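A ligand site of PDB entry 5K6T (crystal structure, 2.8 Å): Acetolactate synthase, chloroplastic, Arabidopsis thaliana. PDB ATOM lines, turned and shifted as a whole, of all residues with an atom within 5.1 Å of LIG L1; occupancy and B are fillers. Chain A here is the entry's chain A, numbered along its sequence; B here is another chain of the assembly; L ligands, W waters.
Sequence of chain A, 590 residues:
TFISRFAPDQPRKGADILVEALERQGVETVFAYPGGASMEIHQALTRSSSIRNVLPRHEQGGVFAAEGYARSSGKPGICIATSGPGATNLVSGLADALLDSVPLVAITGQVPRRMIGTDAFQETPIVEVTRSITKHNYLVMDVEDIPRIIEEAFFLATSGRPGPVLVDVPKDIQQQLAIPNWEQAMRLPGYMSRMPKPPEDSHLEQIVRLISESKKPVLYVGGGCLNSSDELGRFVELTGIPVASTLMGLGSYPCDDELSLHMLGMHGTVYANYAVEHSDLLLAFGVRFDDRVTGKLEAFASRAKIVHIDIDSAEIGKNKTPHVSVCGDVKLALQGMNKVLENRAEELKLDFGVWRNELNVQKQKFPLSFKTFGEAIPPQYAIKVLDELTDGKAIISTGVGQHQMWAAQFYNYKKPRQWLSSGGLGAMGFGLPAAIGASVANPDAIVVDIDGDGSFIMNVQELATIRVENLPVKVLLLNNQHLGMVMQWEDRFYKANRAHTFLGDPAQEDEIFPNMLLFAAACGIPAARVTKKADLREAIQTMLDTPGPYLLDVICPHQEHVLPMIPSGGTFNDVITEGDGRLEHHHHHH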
ATOM      1  N   MET A 266     -11.614  25.128 -23.036  1.00  0.00           N
ATOM      2  CA  MET A 266     -12.989  25.119 -23.533  1.00  0.00           C
ATOM      3  C   MET A 266     -13.103  25.795 -24.896  1.00  0.00           C
ATOM      4  O   MET A 266     -13.776  25.283 -25.783  1.00  0.00           O
ATOM      5  CB  MET A 266     -13.909  25.811 -22.520  1.00  0.00           C
ATOM      6  CG  MET A 266     -15.353  25.933 -22.971  1.00  0.00           C
ATOM      7  SD  MET A 266     -16.458  26.379 -21.608  1.00  0.00           S
ATOM      8  CE  MET A 266     -16.259  24.950 -20.550  1.00  0.00           C
ATOM      9  N   HIS A 267     -12.441  26.933 -25.049  1.00  0.00           N
ATOM     10  CA  HIS A 267     -12.433  27.620 -26.339  1.00  0.00           C
ATOM     11  C   HIS A 267     -11.014  27.709 -26.884  1.00  0.00           C
ATOM     12  O   HIS A 267     -10.676  28.643 -27.614  1.00  0.00           O
ATOM     13  CB  HIS A 267     -13.040  29.019 -26.205  1.00  0.00           C
ATOM     14  CG  HIS A 267     -14.518  29.001 -25.955  1.00  0.00           C
ATOM     15  ND1 HIS A 267     -15.400  28.394 -26.823  1.00  0.00           N
ATOM     16  CD2 HIS A 267     -15.261  29.503 -24.952  1.00  0.00           C
ATOM     17  CE1 HIS A 267     -16.630  28.530 -26.354  1.00  0.00           C
ATOM     18  NE2 HIS A 267     -16.574  29.199 -25.223  1.00  0.00           N
ATOM     19  N   ASP A 291     -11.171  24.044 -14.485  1.00  0.00           N
ATOM     20  CA  ASP A 291     -12.179  23.244 -15.185  1.00  0.00           C
ATOM     21  C   ASP A 291     -12.424  23.729 -16.620  1.00  0.00           C
ATOM     22  O   ASP A 291     -12.853  22.963 -17.470  1.00  0.00           O
ATOM     23  CB  ASP A 291     -13.494  23.216 -14.406  1.00  0.00           C
ATOM     24  CG  ASP A 291     -14.152  24.585 -14.298  1.00  0.00           C
ATOM     25  OD1 ASP A 291     -13.882  25.301 -13.312  1.00  0.00           O
ATOM     26  OD2 ASP A 291     -14.939  24.935 -15.195  1.00  0.00           O
ATOM     27  N   ARG A 292     -12.143  25.014 -16.877  1.00  0.00           N
ATOM     28  CA  ARG A 292     -12.245  25.546 -18.230  1.00  0.00           C
ATOM     29  C   ARG A 292     -11.223  24.883 -19.140  1.00  0.00           C
ATOM     30  O   ARG A 292     -11.408  24.778 -20.350  1.00  0.00           O
ATOM     31  CB  ARG A 292     -12.037  27.069 -18.246  1.00  0.00           C
ATOM     32  CG  ARG A 292     -13.046  27.890 -17.455  1.00  0.00           C
ATOM     33  CD  ARG A 292     -14.457  27.738 -17.998  1.00  0.00           C
ATOM     34  NE  ARG A 292     -15.232  26.775 -17.232  1.00  0.00           N
ATOM     35  CZ  ARG A 292     -16.532  26.581 -17.380  1.00  0.00           C
ATOM     36  NH1 ARG A 292     -17.168  25.676 -16.636  1.00  0.00           N
ATOM     37  NH2 ARG A 292     -17.209  27.286 -18.278  1.00  0.00           N
ATOM     38  N   MET A 405     -13.057  36.058 -25.754  1.00  0.00           N
ATOM     39  CA  MET A 405     -12.452  34.875 -26.347  1.00  0.00           C
ATOM     40  C   MET A 405     -11.810  35.185 -27.689  1.00  0.00           C
ATOM     41  O   MET A 405     -10.705  34.720 -27.982  1.00  0.00           O
ATOM     42  CB  MET A 405     -13.508  33.771 -26.508  1.00  0.00           C
ATOM     43  CG  MET A 405     -14.106  33.289 -25.185  1.00  0.00           C
ATOM     44  SD  MET A 405     -12.914  32.465 -24.112  1.00  0.00           S
ATOM     45  CE  MET A 405     -12.363  33.810 -23.056  1.00  0.00           C
ATOM     46  N   MET A 485     -22.303  35.572 -25.080  1.00  0.00           N
ATOM     47  CA  MET A 485     -21.997  34.224 -24.604  1.00  0.00           C
ATOM     48  C   MET A 485     -23.218  33.501 -24.032  1.00  0.00           C
ATOM     49  O   MET A 485     -23.430  32.320 -24.313  1.00  0.00           O
ATOM     50  CB  MET A 485     -20.892  34.292 -23.538  1.00  0.00           C
ATOM     51  CG  MET A 485     -20.372  32.929 -23.129  1.00  0.00           C
ATOM     52  SD  MET A 485     -19.586  32.054 -24.491  1.00  0.00           S
ATOM     53  CE  MET A 485     -18.180  33.131 -24.805  1.00  0.00           C
ATOM     54  N   VAL A 486     -24.012  34.208 -23.229  1.00  0.00           N
ATOM     55  CA  VAL A 486     -25.239  33.648 -22.678  1.00  0.00           C
ATOM     56  C   VAL A 486     -26.204  33.297 -23.796  1.00  0.00           C
ATOM     57  O   VAL A 486     -26.851  32.250 -23.785  1.00  0.00           O
ATOM     58  CB  VAL A 486     -25.929  34.618 -21.691  1.00  0.00           C
ATOM     59  CG1 VAL A 486     -27.240  34.038 -21.178  1.00  0.00           C
ATOM     60  CG2 VAL A 486     -24.997  34.937 -20.525  1.00  0.00           C
ATOM     61  N   TRP A 489     -25.162  30.074 -25.366  1.00  0.00           N
ATOM     62  CA  TRP A 489     -25.596  28.935 -24.564  1.00  0.00           C
ATOM     63  C   TRP A 489     -27.096  28.704 -24.670  1.00  0.00           C
ATOM     64  O   TRP A 489     -27.574  27.581 -24.520  1.00  0.00           O
ATOM     65  CB  TRP A 489     -25.195  29.136 -23.096  1.00  0.00           C
ATOM     66  CG  TRP A 489     -23.774  28.730 -22.826  1.00  0.00           C
ATOM     67  CD1 TRP A 489     -22.645  29.262 -23.372  1.00  0.00           C
ATOM     68  CD2 TRP A 489     -23.337  27.701 -21.922  1.00  0.00           C
ATOM     69  NE1 TRP A 489     -21.534  28.629 -22.875  1.00  0.00           N
ATOM     70  CE2 TRP A 489     -21.930  27.663 -21.984  1.00  0.00           C
ATOM     71  CE3 TRP A 489     -24.002  26.809 -21.082  1.00  0.00           C
ATOM     72  CZ2 TRP A 489     -21.177  26.769 -21.228  1.00  0.00           C
ATOM     73  CZ3 TRP A 489     -23.249  25.915 -20.326  1.00  0.00           C
ATOM     74  CH2 TRP A 489     -21.853  25.905 -20.410  1.00  0.00           C
ATOM     75  N   SER A 568     -18.933  22.014 -21.052  1.00  0.00           N
ATOM     76  CA  SER A 568     -18.493  21.976 -19.668  1.00  0.00           C
ATOM     77  C   SER A 568     -18.529  20.564 -19.104  1.00  0.00           C
ATOM     78  O   SER A 568     -19.564  19.896 -19.160  1.00  0.00           O
ATOM     79  CB  SER A 568     -19.353  22.912 -18.804  1.00  0.00           C
ATOM     80  OG  SER A 568     -18.863  22.978 -17.481  1.00  0.00           O
ATOM     81  N   GLY B  36     -24.462  32.505 -16.314  1.00  0.00           N
ATOM     82  CA  GLY B  36     -24.409  31.056 -16.453  1.00  0.00           C
ATOM     83  C   GLY B  36     -25.045  30.260 -15.334  1.00  0.00           C
ATOM     84  O   GLY B  36     -25.796  29.308 -15.583  1.00  0.00           O
ATOM     85  N   ALA B  37     -24.762  30.634 -14.093  1.00  0.00           N
ATOM     86  CA  ALA B  37     -25.257  29.891 -12.938  1.00  0.00           C
ATOM     87  C   ALA B  37     -26.734  30.149 -12.667  1.00  0.00           C
ATOM     88  O   ALA B  37     -27.343  29.473 -11.847  1.00  0.00           O
ATOM     89  CB  ALA B  37     -24.428  30.221 -11.703  1.00  0.00           C
ATOM     90  N   MET B  39     -28.998  30.829 -15.461  1.00  0.00           N
ATOM     91  CA  MET B  39     -29.710  30.719 -16.740  1.00  0.00           C
ATOM     92  C   MET B  39     -30.995  29.923 -16.615  1.00  0.00           C
ATOM     93  O   MET B  39     -32.019  30.266 -17.217  1.00  0.00           O
ATOM     94  CB  MET B  39     -28.816  30.086 -17.805  1.00  0.00           C
ATOM     95  CG  MET B  39     -27.739  31.003 -18.349  1.00  0.00           C
ATOM     96  SD  MET B  39     -26.931  30.298 -19.796  1.00  0.00           S
ATOM     97  CE  MET B  39     -28.295  30.276 -20.965  1.00  0.00           C
ATOM     98  N   SER B  83     -23.710  33.728 -10.324  1.00  0.00           N
ATOM     99  CA  SER B  83     -22.638  33.454  -9.377  1.00  0.00           C
ATOM    100  C   SER B  83     -21.474  34.416  -9.547  1.00  0.00           C
ATOM    101  O   SER B  83     -21.461  35.230 -10.472  1.00  0.00           O
ATOM    102  CB  SER B  83     -22.150  32.013  -9.533  1.00  0.00           C
ATOM    103  OG  SER B  83     -21.536  31.822 -10.800  1.00  0.00           O
ATOM    104  N   GLN B 110     -25.427  29.668  -8.214  1.00  0.00           N
ATOM    105  CA  GLN B 110     -24.156  29.158  -7.709  1.00  0.00           C
ATOM    106  C   GLN B 110     -23.681  28.000  -8.579  1.00  0.00           C
ATOM    107  O   GLN B 110     -24.491  27.350  -9.237  1.00  0.00           O
ATOM    108  CB  GLN B 110     -24.296  28.730  -6.245  1.00  0.00           C
ATOM    109  CG  GLN B 110     -23.035  28.163  -5.591  1.00  0.00           C
ATOM    110  CD  GLN B 110     -21.880  29.151  -5.564  1.00  0.00           C
ATOM    111  OE1 GLN B 110     -21.182  29.327  -6.554  1.00  0.00           O
ATOM    112  NE2 GLN B 110     -21.669  29.774  -4.411  1.00  0.00           N
ATOM    113  N   VAL B 111     -22.373  27.767  -8.601  1.00  0.00           N
ATOM    114  CA  VAL B 111     -21.808  26.611  -9.283  1.00  0.00           C
ATOM    115  C   VAL B 111     -22.408  25.318  -8.716  1.00  0.00           C
ATOM    116  O   VAL B 111     -22.927  25.330  -7.599  1.00  0.00           O
ATOM    117  CB  VAL B 111     -20.261  26.578  -9.140  1.00  0.00           C
ATOM    118  CG1 VAL B 111     -19.649  27.847  -9.723  1.00  0.00           C
ATOM    119  CG2 VAL B 111     -19.866  26.410  -7.681  1.00  0.00           C
ATOM    120  N   PRO B 112     -22.364  24.224  -9.488  1.00  0.00           N
ATOM    121  CA  PRO B 112     -22.852  22.926  -9.005  1.00  0.00           C
ATOM    122  C   PRO B 112     -22.274  22.563  -7.636  1.00  0.00           C
ATOM    123  O   PRO B 112     -21.164  22.972  -7.302  1.00  0.00           O
ATOM    124  CB  PRO B 112     -22.365  21.951 -10.073  1.00  0.00           C
ATOM    125  CG  PRO B 112     -22.373  22.767 -11.326  1.00  0.00           C
ATOM    126  CD  PRO B 112     -21.971  24.156 -10.907  1.00  0.00           C
ATOM    127  N   MET B 115     -18.841  21.206  -7.158  1.00  0.00           N
ATOM    128  CA  MET B 115     -17.816  22.134  -7.629  1.00  0.00           C
ATOM    129  C   MET B 115     -17.470  23.179  -6.569  1.00  0.00           C
ATOM    130  O   MET B 115     -16.479  23.899  -6.702  1.00  0.00           O
ATOM    131  CB  MET B 115     -18.271  22.818  -8.919  1.00  0.00           C
ATOM    132  CG  MET B 115     -17.207  22.906  -9.985  1.00  0.00           C
ATOM    133  SD  MET B 115     -16.742  21.303 -10.653  1.00  0.00           S
ATOM    134  CE  MET B 115     -18.318  20.746 -11.297  1.00  0.00           C
ATOM    135  N   ALA B 120     -13.754  27.167  -8.456  1.00  0.00           N
ATOM    136  CA  ALA B 120     -14.298  26.892  -9.782  1.00  0.00           C
ATOM    137  C   ALA B 120     -14.562  28.160 -10.578  1.00  0.00           C
ATOM    138  O   ALA B 120     -14.388  29.278 -10.084  1.00  0.00           O
ATOM    139  CB  ALA B 120     -15.565  26.070  -9.663  1.00  0.00           C
ATOM    140  N   PHE B 121     -15.003  27.974 -11.820  1.00  0.00           N
ATOM    141  CA  PHE B 121     -15.327  29.084 -12.712  1.00  0.00           C
ATOM    142  C   PHE B 121     -16.463  29.934 -12.162  1.00  0.00           C
ATOM    143  O   PHE B 121     -17.563  29.434 -11.918  1.00  0.00           O
ATOM    144  CB  PHE B 121     -15.677  28.548 -14.105  1.00  0.00           C
ATOM    145  CG  PHE B 121     -16.039  29.621 -15.092  1.00  0.00           C
ATOM    146  CD1 PHE B 121     -15.086  30.533 -15.522  1.00  0.00           C
ATOM    147  CD2 PHE B 121     -17.328  29.709 -15.604  1.00  0.00           C
ATOM    148  CE1 PHE B 121     -15.418  31.523 -16.432  1.00  0.00           C
ATOM    149  CE2 PHE B 121     -17.665  30.690 -16.512  1.00  0.00           C
ATOM    150  CZ  PHE B 121     -16.707  31.600 -16.934  1.00  0.00           C
ATOM    151  N   GLN B 122     -16.175  31.221 -11.970  1.00  0.00           N
ATOM    152  CA  GLN B 122     -17.148  32.185 -11.453  1.00  0.00           C
ATOM    153  C   GLN B 122     -17.732  31.760 -10.096  1.00  0.00           C
ATOM    154  O   GLN B 122     -18.941  31.827  -9.894  1.00  0.00           O
ATOM    155  CB  GLN B 122     -18.285  32.399 -12.450  1.00  0.00           C
ATOM    156  CG  GLN B 122     -17.834  32.986 -13.771  1.00  0.00           C
ATOM    157  CD  GLN B 122     -19.003  33.442 -14.627  1.00  0.00           C
ATOM    158  OE1 GLN B 122     -20.036  32.782 -14.706  1.00  0.00           O
ATOM    159  NE2 GLN B 122     -18.835  34.584 -15.283  1.00  0.00           N
ATOM    160  N   LYS B 171     -26.377  25.358  -9.370  1.00  0.00           N
ATOM    161  CA  LYS B 171     -26.957  25.171 -10.695  1.00  0.00           C
ATOM    162  C   LYS B 171     -27.548  23.776 -10.910  1.00  0.00           C
ATOM    163  O   LYS B 171     -28.560  23.625 -11.595  1.00  0.00           O
ATOM    164  CB  LYS B 171     -25.901  25.449 -11.773  1.00  0.00           C
ATOM    165  CG  LYS B 171     -26.453  25.451 -13.194  1.00  0.00           C
ATOM    166  CD  LYS B 171     -25.424  25.974 -14.181  1.00  0.00           C
ATOM    167  CE  LYS B 171     -25.964  25.930 -15.598  1.00  0.00           C
ATOM    168  NZ  LYS B 171     -24.975  26.430 -16.591  1.00  0.00           N
HETATM  169  O1  LIG L   1     -19.638  26.107 -17.038  1.00  0.00           O
HETATM  170  C1  LIG L   1     -20.790  26.595 -17.137  1.00  0.00           C
HETATM  171  N1  LIG L   1     -21.909  25.986 -16.401  1.00  0.00           N
HETATM  172  S1  LIG L   1     -21.621  24.649 -15.457  1.00  0.00           S
HETATM  173  C2  LIG L   1     -20.188  24.892 -14.388  1.00  0.00           C
HETATM  174  C3  LIG L   1     -19.270  23.833 -14.251  1.00  0.00           C
HETATM  175  C4  LIG L   1     -18.157  23.966 -13.452  1.00  0.00           C
HETATM  176  C5  LIG L   1     -17.930  25.163 -12.760  1.00  0.00           C
HETATM  177  C6  LIG L   1     -18.838  26.217 -12.881  1.00  0.00           C
HETATM  178  C7  LIG L   1     -19.967  26.081 -13.695  1.00  0.00           C
HETATM  179  C8  LIG L   1     -20.918  27.255 -13.800  1.00  0.00           C
HETATM  180  O2  LIG L   1     -20.444  28.509 -14.239  1.00  0.00           O
HETATM  181  C9  LIG L   1     -21.453  29.435 -14.529  1.00  0.00           C
HETATM  182  O3  LIG L   1     -22.111  27.119 -13.474  1.00  0.00           O
HETATM  183  O4  LIG L   1     -21.444  23.462 -16.293  1.00  0.00           O
HETATM  184  O5  LIG L   1     -22.798  24.260 -14.691  1.00  0.00           O
HETATM  185  N2  LIG L   1     -20.986  27.737 -17.953  1.00  0.00           N
HETATM  186  N3  LIG L   1     -19.960  28.387 -18.691  1.00  0.00           N
HETATM  187  C10 LIG L   1     -20.547  29.493 -19.392  1.00  0.00           C
HETATM  188  O6  LIG L   1     -19.857  30.380 -20.236  1.00  0.00           O
HETATM  189  C11 LIG L   1     -18.435  30.284 -20.119  1.00  0.00           C
HETATM  190  C12 LIG L   1     -17.893  29.680 -21.427  1.00  0.00           C
HETATM  191  C13 LIG L   1     -17.047  30.675 -22.216  1.00  0.00           C
HETATM  192  N4  LIG L   1     -21.938  29.523 -19.073  1.00  0.00           N
HETATM  193  C14 LIG L   1     -22.873  30.486 -19.582  1.00  0.00           C
HETATM  194  C15 LIG L   1     -22.216  28.445 -18.192  1.00  0.00           C
HETATM  195  O7  LIG L   1     -23.315  28.166 -17.712  1.00  0.00           O
HETATM  196  P1  LG2 L   2      -3.714  31.041 -12.786  1.00  0.00           P
HETATM  197  O1  LG2 L   2      -3.172  32.088 -13.770  1.00  0.00           O
HETATM  198  O2  LG2 L   2      -5.132  31.388 -12.391  1.00  0.00           O
HETATM  199  O3  LG2 L   2      -2.783  31.026 -11.463  1.00  0.00           O
HETATM  200  C1  LG2 L   2      -1.346  30.904 -11.606  1.00  0.00           C
HETATM  201  C2  LG2 L   2      -0.921  29.562 -11.021  1.00  0.00           C
HETATM  202  O4  LG2 L   2       0.498  29.428 -11.084  1.00  0.00           O
HETATM  203  C3  LG2 L   2      -1.290  29.468  -9.580  1.00  0.00           C
HETATM  204  O5  LG2 L   2      -1.587  28.107  -9.250  1.00  0.00           O
HETATM  205  C4  LG2 L   2      -0.087  29.931  -8.873  1.00  0.00           C
HETATM  206  O6  LG2 L   2       0.008  29.307  -7.581  1.00  0.00           O
HETATM  207  C5  LG2 L   2       1.020  29.500  -9.731  1.00  0.00           C
HETATM  208  N1  LG2 L   2       2.084  30.427  -9.713  1.00  0.00           N
HETATM  209  C6  LG2 L   2       1.994  31.748  -9.602  1.00  0.00           C
HETATM  210  N2  LG2 L   2       3.217  32.281  -9.633  1.00  0.00           N
HETATM  211  C7  LG2 L   2       4.138  31.278  -9.761  1.00  0.00           C
HETATM  212  C8  LG2 L   2       5.552  31.181  -9.847  1.00  0.00           C
HETATM  213  N3  LG2 L   2       6.339  32.335  -9.805  1.00  0.00           N
HETATM  214  N4  LG2 L   2       6.134  29.974  -9.981  1.00  0.00           N
HETATM  215  C9  LG2 L   2       5.404  28.880 -10.016  1.00  0.00           C
HETATM  216  N5  LG2 L   2       4.072  28.916  -9.940  1.00  0.00           N
HETATM  217  C10 LG2 L   2       3.411  30.079  -9.818  1.00  0.00           C
HETATM  218  N6  LG2 L   2      -8.916  29.556 -19.680  1.00  0.00           N
HETATM  219  C11 LG2 L   2      -8.294  28.704 -20.625  1.00  0.00           C
HETATM  220  O7  LG2 L   2      -7.138  28.359 -20.461  1.00  0.00           O
HETATM  221  N7  LG2 L   2      -8.986  28.258 -21.738  1.00  0.00           N
HETATM  222  C12 LG2 L   2     -10.291  28.642 -21.929  1.00  0.00           C
HETATM  223  O8  LG2 L   2     -10.900  28.245 -22.908  1.00  0.00           O
HETATM  224  C13 LG2 L   2     -10.986  29.557 -20.930  1.00  0.00           C
HETATM  225  N8  LG2 L   2     -12.299  29.963 -21.098  1.00  0.00           N
HETATM  226  C14 LG2 L   2     -12.744  31.038 -20.382  1.00  0.00           C
HETATM  227  C15 LG2 L   2     -13.927  31.701 -20.775  1.00  0.00           C
HETATM  228  C16 LG2 L   2     -14.379  32.809 -20.044  1.00  0.00           C
HETATM  229  C17 LG2 L   2     -15.671  33.531 -20.473  1.00  0.00           C
HETATM  230  C18 LG2 L   2     -13.659  33.247 -18.928  1.00  0.00           C
HETATM  231  C19 LG2 L   2     -14.169  34.467 -18.139  1.00  0.00           C
HETATM  232  C20 LG2 L   2     -12.482  32.600 -18.539  1.00  0.00           C
HETATM  233  C21 LG2 L   2     -12.029  31.479 -19.274  1.00  0.00           C
HETATM  234  N9  LG2 L   2     -10.868  30.829 -18.900  1.00  0.00           N
HETATM  235  C22 LG2 L   2     -10.276  29.987 -19.835  1.00  0.00           C
HETATM  236  C23 LG2 L   2     -10.086  31.291 -17.827  1.00  0.00           C
HETATM  237  C24 LG2 L   2     -10.055  30.244 -16.682  1.00  0.00           C
HETATM  238  O9  LG2 L   2     -11.271  30.361 -15.947  1.00  0.00           O
HETATM  239  C25 LG2 L   2      -8.847  30.509 -15.708  1.00  0.00           C
HETATM  240  O10 LG2 L   2      -8.742  31.843 -15.497  1.00  0.00           O
HETATM  241  C26 LG2 L   2      -7.557  29.979 -16.285  1.00  0.00           C
HETATM  242  O11 LG2 L   2      -7.794  28.822 -17.080  1.00  0.00           O
HETATM  243  C27 LG2 L   2      -6.637  29.607 -15.148  1.00  0.00           C
HETATM  244  O12 LG2 L   2      -5.371  30.179 -15.365  1.00  0.00           O
HETATM  245  P2  LG2 L   2      -4.079  29.320 -14.929  1.00  0.00           P
HETATM  246  O13 LG2 L   2      -4.403  27.823 -15.051  1.00  0.00           O
HETATM  247  O14 LG2 L   2      -2.923  29.661 -15.868  1.00  0.00           O
HETATM  248  O15 LG2 L   2      -3.656  29.631 -13.454  1.00  0.00           O
HETATM  249  N1  LG3 L   3     -22.516  39.604 -14.722  1.00  0.00           N
HETATM  250  C1  LG3 L   3     -21.226  39.985 -14.462  1.00  0.00           C
HETATM  251  C2  LG3 L   3     -20.935  41.258 -13.628  1.00  0.00           C
HETATM  252  N2  LG3 L   3     -20.179  39.248 -14.934  1.00  0.00           N
HETATM  253  C3  LG3 L   3     -20.421  38.130 -15.666  1.00  0.00           C
HETATM  254  N3  LG3 L   3     -19.321  37.366 -16.143  1.00  0.00           N
HETATM  255  C4  LG3 L   3     -21.716  37.738 -15.938  1.00  0.00           C
HETATM  256  C5  LG3 L   3     -22.758  38.486 -15.454  1.00  0.00           C
HETATM  257  C6  LG3 L   3     -21.980  36.487 -16.745  1.00  0.00           C
HETATM  258  N4  LG3 L   3     -21.714  36.686 -18.151  1.00  0.00           N
HETATM  259  C7  LG3 L   3     -20.708  36.030 -18.926  1.00  0.00           C
HETATM  260  O1  LG3 L   3     -20.125  34.973 -18.649  1.00  0.00           O
HETATM  261  S1  LG3 L   3     -20.468  36.902 -20.187  1.00  0.00           S
HETATM  262  C8  LG3 L   3     -21.724  37.754 -20.342  1.00  0.00           C
HETATM  263  C9  LG3 L   3     -22.486  37.634 -19.123  1.00  0.00           C
HETATM  264  C10 LG3 L   3     -23.820  38.314 -18.828  1.00  0.00           C
HETATM  265  C11 LG3 L   3     -22.123  38.595 -21.560  1.00  0.00           C
HETATM  266  C12 LG3 L   3     -21.251  39.778 -21.734  1.00  0.00           C
HETATM  267  O2  LG3 L   3     -21.841  40.629 -22.729  1.00  0.00           O
HETATM  268  P1  LG3 L   3     -20.945  41.521 -23.631  1.00  0.00           P
HETATM  269  O3  LG3 L   3     -19.875  40.616 -24.363  1.00  0.00           O
HETATM  270  O4  LG3 L   3     -20.229  42.515 -22.785  1.00  0.00           O
HETATM  271  O5  LG3 L   3     -21.792  42.232 -24.638  1.00  0.00           O
HETATM  272  P2  LG3 L   3     -20.198  39.553 -25.504  1.00  0.00           P
HETATM  273  O6  LG3 L   3     -20.488  38.222 -24.875  1.00  0.00           O
HETATM  274  O7  LG3 L   3     -21.394  40.013 -26.305  1.00  0.00           O
HETATM  275  O8  LG3 L   3     -18.986  39.448 -26.416  1.00  0.00           O
HETATM  276  O   HOH W   1     -22.910  22.004 -18.550  1.00  0.00           O
HETATM  277  O   HOH W   2     -19.071  28.584 -24.260  1.00  0.00           O
HETATM  278  O   HOH W   3     -24.298  21.606 -14.827  1.00  0.00           O
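The guanidinium group (NH1) of Arg 292 sits at hydrogen-bond distance from an oxygen (O1) of LIG L1 (2.5 Å). An oxygen (O7) of LIG L1 lies within hydrogen-bond range of the side-chain amino group of Lys 171 of chain B. The side-chain hydroxyl of Ser 568 is in hydrogen-bond range of an oxygen (O4) of LIG L1. O8 of LG2 L2 is in hydrogen-bond range of N of His 267, 2.9 Å away. The backbone NH (N) of Met 266 is in hydrogen-bond range of an oxygen (O8) of LG2 L2, at 3.2 Å. N3 of LG3 L3 sits close to NE2 of Gln 122 of chain B (3.0 Å). An oxygen (O6) of LG3 L3 lies within hydrogen-bond range of the backbone NH (N) of Met 485, at 3.2 Å.
Water W2 lies within hydrogen-bond range of NE2 of His 267, NE1 of Trp 489 and SD of Met 485.
O of Gly 36 of chain B sits close to O7 of LIG L1 (3.5 Å). Merely in contact with LIG L1: Met 266 (3.6 Å), His 267 (3.4 Å), Asp 291 (3.8 Å), Met 485 (3.7 Å), Trp 489 (3.2 Å), Ala 37 of chain B (3.5 Å), Val 111 of chain B (3.6 Å), Pro 112 of chain B (3.7 Å), Met 115 of chain B (3.6 Å), Phe 121 of chain B (3.6 Å) and Gln 122 of chain B (3.6 Å). Hydrophobic or aromatic side chains that line LIG L1: Met 266, His 267, Met 485, Trp 489, Val 111 of chain B, Pro 112 of chain B, Met 115 of chain B and Phe 121 of chain B. Along chain A the residues within 4 Å of LIG L1 span positions 266 to 568. The nearest printed residue that does not touch LIG L1 is Ala 120 of chain B (4.001 Å).
The side-chain hydroxyl (OG) of Ser 568 is in hydrogen-bond range of the guanidinium group (NH1) of Arg 292. The backbone carbonyl oxygen of Arg 292 sits at hydrogen-bond distance from the backbone NH of Met 266 (2.7 Å). NH1 of Arg 292 lies within salt-bridge range of OD2 of Asp 291 (2.8 Å). The side-chain amino group (NZ) of Lys 171 of chain B lies within hydrogen-bond range of the backbone carbonyl oxygen (O) of Gly 36 of chain B, at 3.2 Å. The side-chain carboxylate (OD1) of Asp 291 is in hydrogen-bond range of the backbone NH (N) of Phe 121 of chain B, 3.3 Å away. OG of Ser 83 of chain B lies within hydrogen-bond range of O of Gln 122 of chain B, at 2.7 Å.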
